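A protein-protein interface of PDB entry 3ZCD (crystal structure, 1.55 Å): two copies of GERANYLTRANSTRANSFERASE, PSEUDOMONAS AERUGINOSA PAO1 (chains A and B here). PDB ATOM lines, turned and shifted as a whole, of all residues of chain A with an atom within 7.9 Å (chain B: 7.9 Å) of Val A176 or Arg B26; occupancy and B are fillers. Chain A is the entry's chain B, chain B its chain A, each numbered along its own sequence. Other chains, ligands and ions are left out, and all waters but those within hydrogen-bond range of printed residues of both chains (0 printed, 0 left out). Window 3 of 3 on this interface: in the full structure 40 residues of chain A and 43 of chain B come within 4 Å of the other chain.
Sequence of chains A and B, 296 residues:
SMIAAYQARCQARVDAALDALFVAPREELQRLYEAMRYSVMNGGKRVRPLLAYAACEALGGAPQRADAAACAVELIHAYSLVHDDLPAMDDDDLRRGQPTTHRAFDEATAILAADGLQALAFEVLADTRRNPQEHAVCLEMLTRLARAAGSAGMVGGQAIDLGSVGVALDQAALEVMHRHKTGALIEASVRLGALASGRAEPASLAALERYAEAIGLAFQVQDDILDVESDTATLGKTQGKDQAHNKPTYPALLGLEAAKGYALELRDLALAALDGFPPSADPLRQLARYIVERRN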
ATOM      1  N   SER A 151       9.204  -9.164   4.035  1.00  0.00           N
ATOM      2  CA  SER A 151       9.027  -8.618   2.698  1.00  0.00           C
ATOM      3  C   SER A 151       7.583  -8.413   2.230  1.00  0.00           C
ATOM      4  O   SER A 151       7.314  -7.758   1.235  1.00  0.00           O
ATOM      5  CB  SER A 151       9.747  -9.517   1.704  1.00  0.00           C
ATOM      6  OG  SER A 151      11.167  -9.519   1.893  1.00  0.00           O
ATOM      7  N   ALA A 152       6.622  -8.947   3.006  1.00  0.00           N
ATOM      8  CA  ALA A 152       5.206  -8.729   2.727  1.00  0.00           C
ATOM      9  C   ALA A 152       4.660  -7.576   3.529  1.00  0.00           C
ATOM     10  O   ALA A 152       3.445  -7.264   3.420  1.00  0.00           O
ATOM     11  CB  ALA A 152       4.433  -9.983   3.013  1.00  0.00           C
ATOM     12  N   GLY A 153       5.518  -7.001   4.363  1.00  0.00           N
ATOM     13  CA  GLY A 153       5.161  -5.904   5.275  1.00  0.00           C
ATOM     14  C   GLY A 153       6.177  -4.773   5.143  1.00  0.00           C
ATOM     15  O   GLY A 153       6.343  -4.176   4.051  1.00  0.00           O
ATOM     16  N   GLY A 156       8.874  -4.918   2.516  1.00  0.00           N
ATOM     17  CA  GLY A 156       8.098  -4.755   1.293  1.00  0.00           C
ATOM     18  C   GLY A 156       7.820  -3.289   1.007  1.00  0.00           C
ATOM     19  O   GLY A 156       8.039  -2.770  -0.122  1.00  0.00           O
ATOM     20  N   GLY A 157       7.361  -2.552   2.028  1.00  0.00           N
ATOM     21  CA  GLY A 157       7.040  -1.145   1.833  1.00  0.00           C
ATOM     22  C   GLY A 157       8.245  -0.319   1.418  1.00  0.00           C
ATOM     23  O   GLY A 157       8.124   0.620   0.647  1.00  0.00           O
ATOM     24  N   ILE A 160       8.760  -0.964  -2.193  1.00  0.00           N
ATOM     25  CA  ILE A 160       7.772  -0.279  -3.001  1.00  0.00           C
ATOM     26  C   ILE A 160       8.188   1.190  -3.164  1.00  0.00           C
ATOM     27  O   ILE A 160       7.973   1.782  -4.199  1.00  0.00           O
ATOM     28  CB  ILE A 160       6.333  -0.412  -2.415  1.00  0.00           C
ATOM     29  CG1 ILE A 160       5.880  -1.872  -2.438  1.00  0.00           C
ATOM     30  CG2 ILE A 160       5.325   0.464  -3.179  1.00  0.00           C
ATOM     31  CD1 ILE A 160       4.536  -2.130  -1.754  1.00  0.00           C
ATOM     32  N   LEU A 169       2.708   9.062  -7.660  1.00  0.00           N
ATOM     33  CA  LEU A 169       1.788   8.115  -7.060  1.00  0.00           C
ATOM     34  C   LEU A 169       0.421   8.775  -6.956  1.00  0.00           C
ATOM     35  O   LEU A 169       0.302   9.937  -6.563  1.00  0.00           O
ATOM     36  CB  LEU A 169       2.278   7.633  -5.690  1.00  0.00           C
ATOM     37  CG  LEU A 169       3.568   6.796  -5.667  1.00  0.00           C
ATOM     38  CD1 LEU A 169       3.822   6.286  -4.252  1.00  0.00           C
ATOM     39  CD2 LEU A 169       3.511   5.639  -6.656  1.00  0.00           C
ATOM     40  N   ASP A 170      -0.607   8.049  -7.363  1.00  0.00           N
ATOM     41  CA  ASP A 170      -1.949   8.459  -7.044  1.00  0.00           C
ATOM     42  C   ASP A 170      -2.194   8.055  -5.587  1.00  0.00           C
ATOM     43  O   ASP A 170      -1.339   7.400  -4.947  1.00  0.00           O
ATOM     44  CB  ASP A 170      -3.001   7.957  -8.070  1.00  0.00           C
ATOM     45  CG  ASP A 170      -3.192   6.459  -8.076  1.00  0.00           C
ATOM     46  OD1 ASP A 170      -2.538   5.767  -7.274  1.00  0.00           O
ATOM     47  OD2 ASP A 170      -4.019   5.973  -8.888  1.00  0.00           O
ATOM     48  N   GLN A 171      -3.325   8.479  -5.045  1.00  0.00           N
ATOM     49  CA  GLN A 171      -3.584   8.253  -3.627  1.00  0.00           C
ATOM     50  C   GLN A 171      -3.581   6.756  -3.287  1.00  0.00           C
ATOM     51  O   GLN A 171      -2.991   6.344  -2.289  1.00  0.00           O
ATOM     52  CB  GLN A 171      -4.890   8.872  -3.204  1.00  0.00           C
ATOM     53  CG  GLN A 171      -5.104   8.735  -1.717  1.00  0.00           C
ATOM     54  CD  GLN A 171      -6.275   9.538  -1.207  1.00  0.00           C
ATOM     55  OE1 GLN A 171      -6.867  10.328  -1.934  1.00  0.00           O
ATOM     56  NE2 GLN A 171      -6.606   9.346   0.053  1.00  0.00           N
ATOM     57  N   ALA A 172      -4.226   5.952  -4.128  1.00  0.00           N
ATOM     58  CA  ALA A 172      -4.295   4.499  -3.910  1.00  0.00           C
ATOM     59  C   ALA A 172      -2.903   3.872  -3.807  1.00  0.00           C
ATOM     60  O   ALA A 172      -2.641   3.075  -2.931  1.00  0.00           O
ATOM     61  CB  ALA A 172      -5.108   3.822  -5.012  1.00  0.00           C
ATOM     62  N   ALA A 173      -2.010   4.235  -4.725  1.00  0.00           N
ATOM     63  CA  ALA A 173      -0.647   3.659  -4.749  1.00  0.00           C
ATOM     64  C   ALA A 173       0.163   4.143  -3.540  1.00  0.00           C
ATOM     65  O   ALA A 173       0.940   3.389  -2.950  1.00  0.00           O
ATOM     66  CB  ALA A 173       0.068   3.993  -6.046  1.00  0.00           C
ATOM     67  N   LEU A 174      -0.022   5.417  -3.186  1.00  0.00           N
ATOM     68  CA  LEU A 174       0.634   5.980  -2.009  1.00  0.00           C
ATOM     69  C   LEU A 174       0.215   5.209  -0.760  1.00  0.00           C
ATOM     70  O   LEU A 174       1.068   4.859   0.077  1.00  0.00           O
ATOM     71  CB  LEU A 174       0.282   7.456  -1.849  1.00  0.00           C
ATOM     72  CG  LEU A 174       0.952   8.154  -0.668  1.00  0.00           C
ATOM     73  CD1 LEU A 174       2.450   8.217  -0.889  1.00  0.00           C
ATOM     74  CD2 LEU A 174       0.366   9.553  -0.525  1.00  0.00           C
ATOM     75  N   GLU A 175      -1.092   4.928  -0.657  1.00  0.00           N
ATOM     76  CA  GLU A 175      -1.603   4.228   0.498  1.00  0.00           C
ATOM     77  C   GLU A 175      -1.144   2.774   0.558  1.00  0.00           C
ATOM     78  O   GLU A 175      -0.873   2.245   1.624  1.00  0.00           O
ATOM     79  CB  GLU A 175      -3.125   4.358   0.550  1.00  0.00           C
ATOM     80  CG  GLU A 175      -3.457   5.803   0.888  1.00  0.00           C
ATOM     81  CD  GLU A 175      -4.893   6.107   1.182  1.00  0.00           C
ATOM     82  OE1 GLU A 175      -5.762   5.219   1.035  1.00  0.00           O
ATOM     83  OE2 GLU A 175      -5.123   7.273   1.577  1.00  0.00           O
ATOM     84  N   VAL A 176      -1.062   2.118  -0.587  1.00  0.00           N
ATOM     85  CA  VAL A 176      -0.413   0.795  -0.620  1.00  0.00           C
ATOM     86  C   VAL A 176       1.005   0.859  -0.032  1.00  0.00           C
ATOM     87  O   VAL A 176       1.412   0.004   0.754  1.00  0.00           O
ATOM     88  CB  VAL A 176      -0.389   0.172  -2.013  1.00  0.00           C
ATOM     89  CG1 VAL A 176       0.497  -1.072  -2.021  1.00  0.00           C
ATOM     90  CG2 VAL A 176      -1.794  -0.180  -2.492  1.00  0.00           C
ATOM     91  N   MET A 177       1.778   1.849  -0.456  1.00  0.00           N
ATOM     92  CA  MET A 177       3.142   1.988   0.039  1.00  0.00           C
ATOM     93  C   MET A 177       3.151   2.176   1.552  1.00  0.00           C
ATOM     94  O   MET A 177       3.811   1.449   2.273  1.00  0.00           O
ATOM     95  CB  MET A 177       3.863   3.141  -0.640  1.00  0.00           C
ATOM     96  CG  MET A 177       5.233   3.390  -0.022  1.00  0.00           C
ATOM     97  SD  MET A 177       6.182   4.635  -0.894  1.00  0.00           S
ATOM     98  CE  MET A 177       5.309   6.045  -0.217  1.00  0.00           C
ATOM     99  N   HIS A 178       2.338   3.107   2.028  1.00  0.00           N
ATOM    100  CA  HIS A 178       2.261   3.368   3.467  1.00  0.00           C
ATOM    101  C   HIS A 178       1.768   2.171   4.283  1.00  0.00           C
ATOM    102  O   HIS A 178       2.316   1.916   5.362  1.00  0.00           O
ATOM    103  CB  HIS A 178       1.391   4.574   3.775  1.00  0.00           C
ATOM    104  CG  HIS A 178       2.000   5.872   3.392  1.00  0.00           C
ATOM    105  ND1 HIS A 178       3.331   6.172   3.593  1.00  0.00           N
ATOM    106  CD2 HIS A 178       1.446   6.979   2.857  1.00  0.00           C
ATOM    107  CE1 HIS A 178       3.569   7.403   3.187  1.00  0.00           C
ATOM    108  NE2 HIS A 178       2.441   7.913   2.738  1.00  0.00           N
ATOM    109  N   ARG A 179       0.746   1.478   3.790  1.00  0.00           N
ATOM    110  CA  ARG A 179       0.212   0.298   4.504  1.00  0.00           C
ATOM    111  C   ARG A 179       1.277  -0.727   4.781  1.00  0.00           C
ATOM    112  O   ARG A 179       1.310  -1.362   5.799  1.00  0.00           O
ATOM    113  CB  ARG A 179      -0.955  -0.347   3.769  1.00  0.00           C
ATOM    114  CG  ARG A 179      -2.215   0.477   3.912  1.00  0.00           C
ATOM    115  CD  ARG A 179      -3.539  -0.244   3.618  1.00  0.00           C
ATOM    116  NE  ARG A 179      -3.798  -1.536   4.282  1.00  0.00           N
ATOM    117  CZ  ARG A 179      -3.793  -1.797   5.595  1.00  0.00           C
ATOM    118  NH1 ARG A 179      -3.453  -0.894   6.504  1.00  0.00           N
ATOM    119  NH2 ARG A 179      -4.091  -3.027   6.001  1.00  0.00           N
ATOM    120  N   HIS A 180       2.195  -0.881   3.799  1.00  0.00           N
ATOM    121  CA  HIS A 180       3.275  -1.782   3.987  1.00  0.00           C
ATOM    122  C   HIS A 180       4.395  -1.196   4.837  1.00  0.00           C
ATOM    123  O   HIS A 180       4.896  -1.857   5.742  1.00  0.00           O
ATOM    124  CB  HIS A 180       3.858  -2.172   2.606  1.00  0.00           C
ATOM    125  CG  HIS A 180       2.996  -3.116   1.852  1.00  0.00           C
ATOM    126  ND1 HIS A 180       1.836  -2.725   1.237  1.00  0.00           N
ATOM    127  CD2 HIS A 180       3.116  -4.440   1.621  1.00  0.00           C
ATOM    128  CE1 HIS A 180       1.278  -3.769   0.655  1.00  0.00           C
ATOM    129  NE2 HIS A 180       2.037  -4.822   0.877  1.00  0.00           N
ATOM    130  N   LYS A 181       4.839   0.008   4.497  1.00  0.00           N
ATOM    131  CA  LYS A 181       6.085   0.531   5.046  1.00  0.00           C
ATOM    132  C   LYS A 181       5.960   0.853   6.531  1.00  0.00           C
ATOM    133  O   LYS A 181       6.879   0.622   7.289  1.00  0.00           O
ATOM    134  CB  LYS A 181       6.510   1.760   4.249  1.00  0.00           C
ATOM    135  CG  LYS A 181       7.874   2.268   4.602  1.00  0.00           C
ATOM    136  CD  LYS A 181       8.383   3.223   3.528  1.00  0.00           C
ATOM    137  CE  LYS A 181       7.957   4.642   3.843  1.00  0.00           C
ATOM    138  NZ  LYS A 181       8.778   5.610   3.079  1.00  0.00           N
ATOM    139  N   THR A 182       4.803   1.409   6.904  1.00  0.00           N
ATOM    140  CA  THR A 182       4.570   1.676   8.318  1.00  0.00           C
ATOM    141  C   THR A 182       3.304   1.060   8.835  1.00  0.00           C
ATOM    142  O   THR A 182       3.279   0.768  10.026  1.00  0.00           O
ATOM    143  CB  THR A 182       4.523   3.186   8.620  1.00  0.00           C
ATOM    144  OG1 THR A 182       3.595   3.815   7.752  1.00  0.00           O
ATOM    145  CG2 THR A 182       5.891   3.822   8.415  1.00  0.00           C
ATOM    146  N   GLY A 183       2.311   0.841   7.995  1.00  0.00           N
ATOM    147  CA  GLY A 183       1.017   0.316   8.554  1.00  0.00           C
ATOM    148  C   GLY A 183       1.210  -1.035   9.168  1.00  0.00           C
ATOM    149  O   GLY A 183       0.699  -1.323  10.262  1.00  0.00           O
ATOM    150  N   LEU A 217      -2.447   5.124   9.137  1.00  0.00           N
ATOM    151  CA  LEU A 217      -2.543   6.108   8.074  1.00  0.00           C
ATOM    152  C   LEU A 217      -2.636   7.515   8.619  1.00  0.00           C
ATOM    153  O   LEU A 217      -2.012   8.411   8.067  1.00  0.00           O
ATOM    154  CB  LEU A 217      -3.733   5.816   7.167  1.00  0.00           C
ATOM    155  CG  LEU A 217      -3.649   6.232   5.726  1.00  0.00           C
ATOM    156  CD1 LEU A 217      -2.337   5.719   5.126  1.00  0.00           C
ATOM    157  CD2 LEU A 217      -4.847   5.665   4.973  1.00  0.00           C
ATOM    158  N   TYR A 250       0.544  13.863   1.343  1.00  0.00           N
ATOM    159  CA  TYR A 250      -0.894  14.040   1.315  1.00  0.00           C
ATOM    160  C   TYR A 250      -1.292  15.459   0.939  1.00  0.00           C
ATOM    161  O   TYR A 250      -2.219  15.633   0.144  1.00  0.00           O
ATOM    162  CB  TYR A 250      -1.533  13.580   2.625  1.00  0.00           C
ATOM    163  CG  TYR A 250      -1.728  12.086   2.597  1.00  0.00           C
ATOM    164  CD1 TYR A 250      -2.844  11.521   1.967  1.00  0.00           C
ATOM    165  CD2 TYR A 250      -0.777  11.236   3.124  1.00  0.00           C
ATOM    166  CE1 TYR A 250      -3.024  10.165   1.882  1.00  0.00           C
ATOM    167  CE2 TYR A 250      -0.947   9.858   3.037  1.00  0.00           C
ATOM    168  CZ  TYR A 250      -2.071   9.341   2.421  1.00  0.00           C
ATOM    169  OH  TYR A 250      -2.268   8.004   2.342  1.00  0.00           O
ATOM    170  N   VAL B  23       7.013 -16.220  -3.587  1.00  0.00           N
ATOM    171  CA  VAL B  23       5.920 -15.688  -4.376  1.00  0.00           C
ATOM    172  C   VAL B  23       5.492 -14.331  -3.786  1.00  0.00           C
ATOM    173  O   VAL B  23       4.955 -14.254  -2.676  1.00  0.00           O
ATOM    174  CB  VAL B  23       4.727 -16.672  -4.420  1.00  0.00           C
ATOM    175  CG1 VAL B  23       3.540 -16.076  -5.161  1.00  0.00           C
ATOM    176  CG2 VAL B  23       5.145 -17.987  -5.070  1.00  0.00           C
ATOM    177  N   ALA B  24       5.732 -13.269  -4.541  1.00  0.00           N
ATOM    178  CA  ALA B  24       5.282 -11.920  -4.145  1.00  0.00           C
ATOM    179  C   ALA B  24       3.774 -11.911  -3.969  1.00  0.00           C
ATOM    180  O   ALA B  24       3.038 -12.358  -4.828  1.00  0.00           O
ATOM    181  CB  ALA B  24       5.648 -10.904  -5.189  1.00  0.00           C
ATOM    182  N   PRO B  25       3.286 -11.440  -2.803  1.00  0.00           N
ATOM    183  CA  PRO B  25       1.827 -11.378  -2.615  1.00  0.00           C
ATOM    184  C   PRO B  25       1.085 -10.316  -3.424  1.00  0.00           C
ATOM    185  O   PRO B  25      -0.164 -10.325  -3.471  1.00  0.00           O
ATOM    186  CB  PRO B  25       1.669 -11.109  -1.124  1.00  0.00           C
ATOM    187  CG  PRO B  25       2.995 -10.689  -0.634  1.00  0.00           C
ATOM    188  CD  PRO B  25       4.058 -11.009  -1.633  1.00  0.00           C
ATOM    189  N   ARG B  26       1.846  -9.435  -4.075  1.00  0.00           N
ATOM    190  CA  ARG B  26       1.285  -8.484  -5.028  1.00  0.00           C
ATOM    191  C   ARG B  26       2.367  -7.962  -5.951  1.00  0.00           C
ATOM    192  O   ARG B  26       3.551  -8.092  -5.657  1.00  0.00           O
ATOM    193  CB  ARG B  26       0.565  -7.342  -4.322  1.00  0.00           C
ATOM    194  CG  ARG B  26       1.356  -6.637  -3.246  1.00  0.00           C
ATOM    195  CD  ARG B  26       0.410  -5.750  -2.427  1.00  0.00           C
ATOM    196  NE  ARG B  26      -0.233  -4.780  -3.324  1.00  0.00           N
ATOM    197  CZ  ARG B  26      -1.447  -4.253  -3.175  1.00  0.00           C
ATOM    198  NH1 ARG B  26      -2.213  -4.564  -2.131  1.00  0.00           N
ATOM    199  NH2 ARG B  26      -1.883  -3.397  -4.086  1.00  0.00           N
ATOM    200  N   GLU B  27       1.931  -7.371  -7.052  1.00  0.00           N
ATOM    201  CA  GLU B  27       2.803  -7.018  -8.161  1.00  0.00           C
ATOM    202  C   GLU B  27       3.904  -6.025  -7.777  1.00  0.00           C
ATOM    203  O   GLU B  27       5.040  -6.157  -8.200  1.00  0.00           O
ATOM    204  CB  GLU B  27       1.936  -6.510  -9.319  1.00  0.00           C
ATOM    205  CG  GLU B  27       2.685  -5.938 -10.512  1.00  0.00           C
ATOM    206  CD  GLU B  27       1.738  -5.514 -11.627  1.00  0.00           C
ATOM    207  OE1 GLU B  27       0.614  -5.053 -11.308  1.00  0.00           O
ATOM    208  OE2 GLU B  27       2.110  -5.646 -12.819  1.00  0.00           O
ATOM    209  N   GLU B  28       3.586  -5.069  -6.908  1.00  0.00           N
ATOM    210  CA  GLU B  28       4.563  -4.053  -6.500  1.00  0.00           C
ATOM    211  C   GLU B  28       5.812  -4.645  -5.779  1.00  0.00           C
ATOM    212  O   GLU B  28       6.886  -4.008  -5.702  1.00  0.00           O
ATOM    213  CB  GLU B  28       3.895  -2.995  -5.631  1.00  0.00           C
ATOM    214  CG  GLU B  28       2.678  -2.303  -6.253  1.00  0.00           C
ATOM    215  CD  GLU B  28       1.343  -2.920  -5.898  1.00  0.00           C
ATOM    216  OE1 GLU B  28       1.265  -4.139  -5.621  1.00  0.00           O
ATOM    217  OE2 GLU B  28       0.353  -2.171  -5.867  1.00  0.00           O
ATOM    218  N   LEU B  29       5.649  -5.866  -5.260  1.00  0.00           N
ATOM    219  CA  LEU B  29       6.669  -6.554  -4.505  1.00  0.00           C
ATOM    220  C   LEU B  29       7.449  -7.574  -5.355  1.00  0.00           C
ATOM    221  O   LEU B  29       8.316  -8.271  -4.834  1.00  0.00           O
ATOM    222  CB  LEU B  29       6.041  -7.274  -3.313  1.00  0.00           C
ATOM    223  CG  LEU B  29       5.404  -6.339  -2.281  1.00  0.00           C
ATOM    224  CD1 LEU B  29       4.666  -7.170  -1.247  1.00  0.00           C
ATOM    225  CD2 LEU B  29       6.444  -5.453  -1.630  1.00  0.00           C
ATOM    226  N   GLN B  30       7.134  -7.667  -6.657  1.00  0.00           N
ATOM    227  CA  GLN B  30       7.766  -8.683  -7.495  1.00  0.00           C
ATOM    228  C   GLN B  30       9.292  -8.599  -7.537  1.00  0.00           C
ATOM    229  O   GLN B  30       9.962  -9.607  -7.362  1.00  0.00           O
ATOM    230  CB  GLN B  30       7.168  -8.694  -8.905  1.00  0.00           C
ATOM    231  CG  GLN B  30       5.807  -9.393  -8.864  1.00  0.00           C
ATOM    232  CD  GLN B  30       5.032  -9.372 -10.170  1.00  0.00           C
ATOM    233  OE1 GLN B  30       5.461  -8.787 -11.165  1.00  0.00           O
ATOM    234  NE2 GLN B  30       3.875 -10.014 -10.158  1.00  0.00           N
ATOM    235  N   ARG B  31       9.837  -7.401  -7.721  1.00  0.00           N
ATOM    236  CA  ARG B  31      11.284  -7.265  -7.845  1.00  0.00           C
ATOM    237  C   ARG B  31      12.028  -7.639  -6.549  1.00  0.00           C
ATOM    238  O   ARG B  31      12.985  -8.369  -6.505  1.00  0.00           O
ATOM    239  CB  ARG B  31      11.648  -5.860  -8.278  1.00  0.00           C
ATOM    240  CG  ARG B  31      13.111  -5.699  -8.554  1.00  0.00           C
ATOM    241  CD  ARG B  31      13.295  -4.358  -9.213  1.00  0.00           C
ATOM    242  NE  ARG B  31      14.691  -4.077  -9.559  1.00  0.00           N
ATOM    243  CZ  ARG B  31      15.657  -3.590  -8.764  1.00  0.00           C
ATOM    244  NH1 ARG B  31      15.457  -3.321  -7.492  1.00  0.00           N
ATOM    245  NH2 ARG B  31      16.908  -3.374  -9.261  1.00  0.00           N
ATOM    246  N   TYR B  33      10.960  -9.819  -4.284  1.00  0.00           N
ATOM    247  CA  TYR B  33      10.885 -11.248  -4.190  1.00  0.00           C
ATOM    248  C   TYR B  33      11.821 -11.941  -5.148  1.00  0.00           C
ATOM    249  O   TYR B  33      12.416 -12.968  -4.822  1.00  0.00           O
ATOM    250  CB  TYR B  33       9.465 -11.768  -4.314  1.00  0.00           C
ATOM    251  CG  TYR B  33       8.732 -11.680  -2.972  1.00  0.00           C
ATOM    252  CD1 TYR B  33       8.286 -10.458  -2.501  1.00  0.00           C
ATOM    253  CD2 TYR B  33       8.624 -12.787  -2.162  1.00  0.00           C
ATOM    254  CE1 TYR B  33       7.671 -10.337  -1.251  1.00  0.00           C
ATOM    255  CE2 TYR B  33       8.002 -12.676  -0.898  1.00  0.00           C
ATOM    256  CZ  TYR B  33       7.558 -11.456  -0.493  1.00  0.00           C
ATOM    257  OH  TYR B  33       6.911 -11.368   0.759  1.00  0.00           O
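The backbone NH (N) of Ala A152 lies within hydrogen-bond range of the side-chain hydroxyl (OH) of Tyr B33, 3.3 Å away.
The guanidinium group (NE) of Arg B26 is in salt-bridge range of the side-chain carboxylate (OE1) of Glu B28, at 2.8 Å.
O of Ser A151 sits close to N of Gly A156 (3.5 Å).
The backbone carbonyl oxygen (O) of Val A176 sits at hydrogen-bond distance from a ring nitrogen (ND1) of His A180 (2.8 Å).
Printed residues of chain B that touch a printed residue of chain A: Pro B25, Arg B26, Glu B28, Leu B29 and Tyr B33.
Hydrophobic or aromatic side chains of chain B that line the printed part of chain A: Pro B25, Leu B29 and Tyr B33.
Of the 23 printed residues of chain A, 6 touch a printed residue of chain B.
Printed residues of chain A that touch a printed residue of chain B: Ser A151, Ala A152, Gly A156, Ile A160, Val A176 and His A180.
Among the printed residues, 9 pairs touch across the chains.
Among the printed residues, merely in contact across the chains: Ser A151 with Tyr B33 (3.4 Å), Gly A156 with Leu B29 (3.4 Å), Val A176 with Arg B26 (3.6 Å), Ser A151 with Leu B29 (3.7 Å), Ile A160 with Leu B29 (3.7 Å), His A180 with Arg B26 (3.8 Å), Ile A160 with Glu B28 (3.9 Å) and Ala A152 with Pro B25 (3.98 Å).
Of the printed residues of chain B, Ala A152 touches Pro B25 and Tyr B33.
Printed residues of chain B within 4 Å of Ile A160: Glu B28 (3.9 Å) and Leu B29 (3.7 Å).
Printed residues of chain B within 4 Å of Val A176: Arg B26.
Val B23 touches none of the printed residues of chain A.
Of the printed residues of chain A, Pro B25 touches Ala A152 (3.98 Å).
Arg B26 touches just these residues of chain A: Val A176 and His A180.
Of the printed residues of chain A, Leu B29 touches Ser A151 (3.7 Å), Gly A156 (3.4 Å) and Ile A160 (3.7 Å).
The nearest printed residue of chain B that does not touch Val A176 is Glu B28 (4.003 Å).
No position is printed for both chains.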
